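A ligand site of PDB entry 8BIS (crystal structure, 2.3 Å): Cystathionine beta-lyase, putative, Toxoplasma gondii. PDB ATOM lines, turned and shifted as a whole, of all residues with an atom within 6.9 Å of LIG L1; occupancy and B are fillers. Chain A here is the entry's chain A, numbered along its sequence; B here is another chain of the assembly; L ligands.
OH of Tyr 133 lies within hydrogen-bond range of NH2 of Arg 80 of chain B. OD1 of Asn 180 lies within hydrogen-bond range of NH1 of Arg 395, 2.8 Å away. N of Arg 395 lies within hydrogen-bond range of O of Thr 369, 2.9 Å away. The side-chain amino group (NZ) of Lys 230 sits at hydrogen-bond distance from the side-chain hydroxyl (OG) of Ser 227 (3.0 Å).
A carbon (C3) of LIG L1 is covalently linked to the side-chain hydroxyl (OH) of Tyr 133, 1.4 Å away. An oxygen (O1) of LIG L1 is in salt-bridge range of the guanidinium group of Arg 395. NZ of Lys 230 lies close to N1 of LIG L1 (3.2 Å). The backbone NH (N) of Asn 360 is in hydrogen-bond range of an oxygen (O2) of LIG L1, 3.3 Å away. The side-chain amide nitrogen (ND2) of Asn 180 sits at hydrogen-bond distance from an oxygen (O1) of LIG L1 (3.3 Å). A carbon (C5) of LG2 L2 is bonded to the side-chain amino group (NZ) of Lys 230 (1.4 Å). OH of Tyr 78 of chain B sits at hydrogen-bond distance from O4 of LG2 L2, at 2.5 Å. NE of Arg 80 of chain B is in salt-bridge range of O3 of LG2 L2, at 2.9 Å. O2 of LG2 L2 sits at hydrogen-bond distance from OG of Ser 227 (3.0 Å). The backbone NH of Met 109 lies within hydrogen-bond range of an oxygen (O3) of LG2 L2 (2.8 Å).
OE1 of Glu 359 touches C1 of LIG L1, at 3.1 Å. CD2 of Leu 361 touches O1 of LIG L1, 3.7 Å away. Tyr 78 of chain B touches LIG L1 (CG to C1, 3.6 Å). Arg 80 of chain B touches LIG L1 (NH2 to C3, 3.6 Å). Nine residues have an atom within 4 Å of LIG L1: Tyr 133, Asn 180, Lys 230, Glu 359, Asn 360, Leu 361, Arg 395, Tyr 78 of chain B and Arg 80 of chain B. Along chain A the residues within 4 Å of LIG L1 span positions 133 to 395. The nearest printed residue that does not touch LIG L1 is Thr 375 (4.9 Å).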
ATOM      1  N   MET A 109      -0.358  12.522  -0.996  1.00  0.00           N
ATOM      2  CA  MET A 109      -1.433  12.579  -0.017  1.00  0.00           C
ATOM      3  C   MET A 109      -1.480  11.323   0.831  1.00  0.00           C
ATOM      4  O   MET A 109      -1.798  11.383   2.019  1.00  0.00           O
ATOM      5  CB  MET A 109      -2.772  12.800  -0.710  1.00  0.00           C
ATOM      6  CG  MET A 109      -3.054  14.247  -1.063  1.00  0.00           C
ATOM      7  SD  MET A 109      -2.762  15.380   0.304  1.00  0.00           S
ATOM      8  CE  MET A 109      -3.865  14.705   1.545  1.00  0.00           C
ATOM      9  N   TYR A 133      -0.041  22.958   1.610  1.00  0.00           N
ATOM     10  CA  TYR A 133      -0.670  22.470   0.392  1.00  0.00           C
ATOM     11  C   TYR A 133      -2.154  22.245   0.627  1.00  0.00           C
ATOM     12  O   TYR A 133      -2.567  21.775   1.686  1.00  0.00           O
ATOM     13  CB  TYR A 133      -0.005  21.173  -0.065  1.00  0.00           C
ATOM     14  CG  TYR A 133      -0.765  20.508  -1.190  1.00  0.00           C
ATOM     15  CD1 TYR A 133      -1.003  21.196  -2.373  1.00  0.00           C
ATOM     16  CD2 TYR A 133      -1.236  19.210  -1.077  1.00  0.00           C
ATOM     17  CE1 TYR A 133      -1.701  20.612  -3.413  1.00  0.00           C
ATOM     18  CE2 TYR A 133      -1.927  18.615  -2.110  1.00  0.00           C
ATOM     19  CZ  TYR A 133      -2.155  19.324  -3.285  1.00  0.00           C
ATOM     20  OH  TYR A 133      -2.846  18.745  -4.337  1.00  0.00           O
ATOM     21  N   GLY A 134      -2.967  22.616  -0.369  1.00  0.00           N
ATOM     22  CA  GLY A 134      -4.411  22.556  -0.200  1.00  0.00           C
ATOM     23  C   GLY A 134      -4.915  21.186   0.219  1.00  0.00           C
ATOM     24  O   GLY A 134      -5.803  21.078   1.070  1.00  0.00           O
ATOM     25  N   GLY A 135      -4.360  20.129  -0.365  1.00  0.00           N
ATOM     26  CA  GLY A 135      -4.771  18.786   0.002  1.00  0.00           C
ATOM     27  C   GLY A 135      -4.492  18.468   1.464  1.00  0.00           C
ATOM     28  O   GLY A 135      -5.322  17.867   2.150  1.00  0.00           O
ATOM     29  N   ARG A 138      -7.099  20.345   3.578  1.00  0.00           N
ATOM     30  CA  ARG A 138      -8.416  19.729   3.530  1.00  0.00           C
ATOM     31  C   ARG A 138      -8.448  18.404   4.295  1.00  0.00           C
ATOM     32  O   ARG A 138      -9.384  18.147   5.056  1.00  0.00           O
ATOM     33  CB  ARG A 138      -8.841  19.511   2.080  1.00  0.00           C
ATOM     34  CG  ARG A 138      -9.853  18.390   1.901  1.00  0.00           C
ATOM     35  CD  ARG A 138     -10.496  18.440   0.531  1.00  0.00           C
ATOM     36  NE  ARG A 138      -9.538  18.185  -0.546  1.00  0.00           N
ATOM     37  CZ  ARG A 138      -9.888  17.936  -1.799  1.00  0.00           C
ATOM     38  NH1 ARG A 138      -8.951  17.716  -2.716  1.00  0.00           N
ATOM     39  NH2 ARG A 138     -11.169  17.913  -2.145  1.00  0.00           N
ATOM     40  N   ASN A 180       3.144  25.764  -0.712  1.00  0.00           N
ATOM     41  CA  ASN A 180       2.314  25.738  -1.900  1.00  0.00           C
ATOM     42  C   ASN A 180       1.097  26.614  -1.674  1.00  0.00           C
ATOM     43  O   ASN A 180       0.301  26.317  -0.766  1.00  0.00           O
ATOM     44  CB  ASN A 180       1.882  24.316  -2.224  1.00  0.00           C
ATOM     45  CG  ASN A 180       1.269  24.182  -3.618  1.00  0.00           C
ATOM     46  OD1 ASN A 180       0.898  25.165  -4.246  1.00  0.00           O
ATOM     47  ND2 ASN A 180       1.171  22.944  -4.095  1.00  0.00           N
ATOM     48  N   PHE A 208       8.350  21.010  -2.780  1.00  0.00           N
ATOM     49  CA  PHE A 208       8.757  22.107  -3.648  1.00  0.00           C
ATOM     50  C   PHE A 208      10.270  22.302  -3.680  1.00  0.00           C
ATOM     51  O   PHE A 208      10.789  22.890  -4.639  1.00  0.00           O
ATOM     52  CB  PHE A 208       8.113  23.410  -3.185  1.00  0.00           C
ATOM     53  CG  PHE A 208       6.776  23.675  -3.791  1.00  0.00           C
ATOM     54  CD1 PHE A 208       5.836  22.664  -3.926  1.00  0.00           C
ATOM     55  CD2 PHE A 208       6.441  24.941  -4.235  1.00  0.00           C
ATOM     56  CE1 PHE A 208       4.595  22.918  -4.479  1.00  0.00           C
ATOM     57  CE2 PHE A 208       5.206  25.201  -4.800  1.00  0.00           C
ATOM     58  CZ  PHE A 208       4.281  24.191  -4.918  1.00  0.00           C
ATOM     59  N   SER A 227       5.999  14.504  -2.183  1.00  0.00           N
ATOM     60  CA  SER A 227       5.153  14.107  -3.301  1.00  0.00           C
ATOM     61  C   SER A 227       6.089  13.784  -4.453  1.00  0.00           C
ATOM     62  O   SER A 227       6.571  14.695  -5.147  1.00  0.00           O
ATOM     63  CB  SER A 227       4.164  15.210  -3.656  1.00  0.00           C
ATOM     64  OG  SER A 227       3.569  14.927  -4.911  1.00  0.00           O
ATOM     65  N   LYS A 230       5.772  15.129  -8.214  1.00  0.00           N
ATOM     66  CA  LYS A 230       6.197  16.412  -8.758  1.00  0.00           C
ATOM     67  C   LYS A 230       7.581  16.346  -9.390  1.00  0.00           C
ATOM     68  O   LYS A 230       7.703  16.199 -10.611  1.00  0.00           O
ATOM     69  CB  LYS A 230       6.174  17.488  -7.672  1.00  0.00           C
ATOM     70  CG  LYS A 230       4.885  17.534  -6.861  1.00  0.00           C
ATOM     71  CD  LYS A 230       3.660  17.432  -7.744  1.00  0.00           C
ATOM     72  CE  LYS A 230       2.430  17.984  -7.058  1.00  0.00           C
ATOM     73  NZ  LYS A 230       2.427  17.568  -5.635  1.00  0.00           N
ATOM     74  N   CYS A 358      -3.048  23.648 -16.342  1.00  0.00           N
ATOM     75  CA  CYS A 358      -3.379  22.383 -15.679  1.00  0.00           C
ATOM     76  C   CYS A 358      -2.895  22.457 -14.233  1.00  0.00           C
ATOM     77  O   CYS A 358      -2.351  23.477 -13.791  1.00  0.00           O
ATOM     78  CB  CYS A 358      -2.791  21.199 -16.431  1.00  0.00           C
ATOM     79  SG  CYS A 358      -0.983  21.174 -16.453  1.00  0.00           S
ATOM     80  N   GLU A 359      -3.089  21.367 -13.501  1.00  0.00           N
ATOM     81  CA  GLU A 359      -2.557  21.254 -12.151  1.00  0.00           C
ATOM     82  C   GLU A 359      -1.202  20.523 -12.219  1.00  0.00           C
ATOM     83  O   GLU A 359      -0.584  20.485 -13.278  1.00  0.00           O
ATOM     84  CB  GLU A 359      -3.584  20.570 -11.240  1.00  0.00           C
ATOM     85  CG  GLU A 359      -4.816  21.437 -10.982  1.00  0.00           C
ATOM     86  CD  GLU A 359      -6.076  20.632 -10.714  1.00  0.00           C
ATOM     87  OE1 GLU A 359      -6.016  19.657  -9.948  1.00  0.00           O
ATOM     88  OE2 GLU A 359      -7.131  20.983 -11.287  1.00  0.00           O
ATOM     89  N   ASN A 360      -0.741  19.987 -11.095  1.00  0.00           N
ATOM     90  CA  ASN A 360       0.581  19.378 -10.970  1.00  0.00           C
ATOM     91  C   ASN A 360       1.690  20.415 -11.142  1.00  0.00           C
ATOM     92  O   ASN A 360       1.420  21.566 -11.520  1.00  0.00           O
ATOM     93  CB  ASN A 360       0.762  18.239 -11.985  1.00  0.00           C
ATOM     94  CG  ASN A 360       1.875  17.289 -11.615  1.00  0.00           C
ATOM     95  OD1 ASN A 360       2.163  17.086 -10.439  1.00  0.00           O
ATOM     96  ND2 ASN A 360       2.523  16.706 -12.615  1.00  0.00           N
ATOM     97  N   LEU A 361       2.925  20.044 -10.842  1.00  0.00           N
ATOM     98  CA  LEU A 361       4.055  20.968 -10.897  1.00  0.00           C
ATOM     99  C   LEU A 361       5.350  20.165 -10.849  1.00  0.00           C
ATOM    100  O   LEU A 361       5.349  18.968 -10.546  1.00  0.00           O
ATOM    101  CB  LEU A 361       4.012  21.972  -9.737  1.00  0.00           C
ATOM    102  CG  LEU A 361       3.957  21.363  -8.333  1.00  0.00           C
ATOM    103  CD1 LEU A 361       5.322  21.452  -7.651  1.00  0.00           C
ATOM    104  CD2 LEU A 361       2.885  22.032  -7.492  1.00  0.00           C
ATOM    105  N   THR A 369      -0.949  27.947 -13.280  1.00  0.00           N
ATOM    106  CA  THR A 369      -2.273  27.810 -12.677  1.00  0.00           C
ATOM    107  C   THR A 369      -2.588  29.055 -11.876  1.00  0.00           C
ATOM    108  O   THR A 369      -1.700  29.803 -11.453  1.00  0.00           O
ATOM    109  CB  THR A 369      -2.358  26.575 -11.784  1.00  0.00           C
ATOM    110  OG1 THR A 369      -3.708  26.417 -11.330  1.00  0.00           O
ATOM    111  CG2 THR A 369      -1.443  26.711 -10.580  1.00  0.00           C
ATOM    112  N   THR A 375      -7.809  25.741  -8.538  1.00  0.00           N
ATOM    113  CA  THR A 375      -7.675  24.872  -7.376  1.00  0.00           C
ATOM    114  C   THR A 375      -8.665  25.245  -6.285  1.00  0.00           C
ATOM    115  O   THR A 375      -9.251  24.356  -5.650  1.00  0.00           O
ATOM    116  CB  THR A 375      -6.240  24.937  -6.839  1.00  0.00           C
ATOM    117  OG1 THR A 375      -5.317  24.941  -7.931  1.00  0.00           O
ATOM    118  CG2 THR A 375      -5.959  23.738  -5.943  1.00  0.00           C
ATOM    119  N   ARG A 395       0.485  30.629  -9.761  1.00  0.00           N
ATOM    120  CA  ARG A 395       1.579  29.712  -9.489  1.00  0.00           C
ATOM    121  C   ARG A 395       2.149  29.185 -10.799  1.00  0.00           C
ATOM    122  O   ARG A 395       1.394  28.818 -11.713  1.00  0.00           O
ATOM    123  CB  ARG A 395       1.096  28.538  -8.623  1.00  0.00           C
ATOM    124  CG  ARG A 395       2.197  27.584  -8.201  1.00  0.00           C
ATOM    125  CD  ARG A 395       1.626  26.363  -7.476  1.00  0.00           C
ATOM    126  NE  ARG A 395       0.994  25.404  -8.380  1.00  0.00           N
ATOM    127  CZ  ARG A 395       0.269  24.362  -7.981  1.00  0.00           C
ATOM    128  NH1 ARG A 395       0.085  24.139  -6.685  1.00  0.00           N
ATOM    129  NH2 ARG A 395      -0.274  23.544  -8.868  1.00  0.00           N
ATOM    130  N   SER B  77      -8.671  16.229 -14.289  1.00  0.00           N
ATOM    131  CA  SER B  77      -7.783  17.312 -13.884  1.00  0.00           C
ATOM    132  C   SER B  77      -6.529  16.775 -13.224  1.00  0.00           C
ATOM    133  O   SER B  77      -5.430  17.293 -13.440  1.00  0.00           O
ATOM    134  CB  SER B  77      -8.517  18.258 -12.922  1.00  0.00           C
ATOM    135  OG  SER B  77      -8.910  17.566 -11.754  1.00  0.00           O
ATOM    136  N   TYR B  78      -6.675  15.726 -12.410  1.00  0.00           N
ATOM    137  CA  TYR B  78      -5.572  15.194 -11.628  1.00  0.00           C
ATOM    138  C   TYR B  78      -5.859  13.738 -11.332  1.00  0.00           C
ATOM    139  O   TYR B  78      -6.985  13.391 -10.973  1.00  0.00           O
ATOM    140  CB  TYR B  78      -5.381  15.992 -10.339  1.00  0.00           C
ATOM    141  CG  TYR B  78      -4.054  15.780  -9.666  1.00  0.00           C
ATOM    142  CD1 TYR B  78      -3.967  15.093  -8.462  1.00  0.00           C
ATOM    143  CD2 TYR B  78      -2.880  16.289 -10.211  1.00  0.00           C
ATOM    144  CE1 TYR B  78      -2.758  14.897  -7.840  1.00  0.00           C
ATOM    145  CE2 TYR B  78      -1.669  16.103  -9.591  1.00  0.00           C
ATOM    146  CZ  TYR B  78      -1.608  15.407  -8.405  1.00  0.00           C
ATOM    147  OH  TYR B  78      -0.392  15.223  -7.773  1.00  0.00           O
ATOM    148  N   ARG B  80      -4.861  11.571  -9.004  1.00  0.00           N
ATOM    149  CA  ARG B  80      -5.232  11.123  -7.654  1.00  0.00           C
ATOM    150  C   ARG B  80      -6.727  11.179  -7.456  1.00  0.00           C
ATOM    151  O   ARG B  80      -7.292  10.365  -6.716  1.00  0.00           O
ATOM    152  CB  ARG B  80      -4.533  11.970  -6.583  1.00  0.00           C
ATOM    153  CG  ARG B  80      -4.592  11.333  -5.205  1.00  0.00           C
ATOM    154  CD  ARG B  80      -4.574  12.340  -4.056  1.00  0.00           C
ATOM    155  NE  ARG B  80      -3.771  13.521  -4.340  1.00  0.00           N
ATOM    156  CZ  ARG B  80      -4.263  14.756  -4.404  1.00  0.00           C
ATOM    157  NH1 ARG B  80      -5.568  14.957  -4.241  1.00  0.00           N
ATOM    158  NH2 ARG B  80      -3.464  15.777  -4.654  1.00  0.00           N
ATOM    159  N   THR B  81      -7.394  12.119  -8.125  1.00  0.00           N
ATOM    160  CA  THR B  81      -8.842  12.264  -8.031  1.00  0.00           C
ATOM    161  C   THR B  81      -9.560  11.281  -8.948  1.00  0.00           C
ATOM    162  O   THR B  81     -10.492  10.586  -8.515  1.00  0.00           O
ATOM    163  CB  THR B  81      -9.235  13.695  -8.387  1.00  0.00           C
ATOM    164  OG1 THR B  81      -8.326  14.609  -7.756  1.00  0.00           O
ATOM    165  CG2 THR B  81     -10.657  13.982  -7.928  1.00  0.00           C
HETATM  166  C1  LIG L   1      -4.061  18.766  -7.720  1.00  0.00           C
HETATM  167  C2  LIG L   1      -4.104  19.232  -6.504  1.00  0.00           C
HETATM  168  C3  LIG L   1      -2.828  19.214  -5.625  1.00  0.00           C
HETATM  169  C4  LIG L   1      -1.583  19.278  -6.504  1.00  0.00           C
HETATM  170  C5  LIG L   1      -1.372  20.671  -7.077  1.00  0.00           C
HETATM  171  O1  LIG L   1      -0.664  21.487  -6.443  1.00  0.00           O
HETATM  172  O2  LIG L   1      -1.896  21.000  -8.197  1.00  0.00           O
HETATM  173  N1  LIG L   1      -0.414  18.931  -5.763  1.00  0.00           N
HETATM  174  N1  LG2 L   2       2.228  18.356  -0.677  1.00  0.00           N
HETATM  175  C1  LG2 L   2       2.773  19.051  -1.687  1.00  0.00           C
HETATM  176  C2  LG2 L   2       3.656  20.254  -1.361  1.00  0.00           C
HETATM  177  C3  LG2 L   2       2.546  18.732  -2.766  1.00  0.00           C
HETATM  178  O1  LG2 L   2       3.134  19.502  -3.775  1.00  0.00           O
HETATM  179  C4  LG2 L   2       1.682  17.574  -3.146  1.00  0.00           C
HETATM  180  C5  LG2 L   2       1.462  17.245  -4.625  1.00  0.00           C
HETATM  181  C6  LG2 L   2       1.173  16.895  -2.365  1.00  0.00           C
HETATM  182  C7  LG2 L   2       1.353  17.165  -0.993  1.00  0.00           C
HETATM  183  C8  LG2 L   2       0.273  15.722  -2.720  1.00  0.00           C
HETATM  184  O2  LG2 L   2       0.967  14.715  -3.382  1.00  0.00           O
HETATM  185  P1  LG2 L   2       0.054  13.861  -4.442  1.00  0.00           P
HETATM  186  O3  LG2 L   2      -0.969  13.062  -3.679  1.00  0.00           O
HETATM  187  O4  LG2 L   2      -0.663  14.840  -5.336  1.00  0.00           O
HETATM  188  O5  LG2 L   2       0.946  12.959  -5.246  1.00  0.00           O
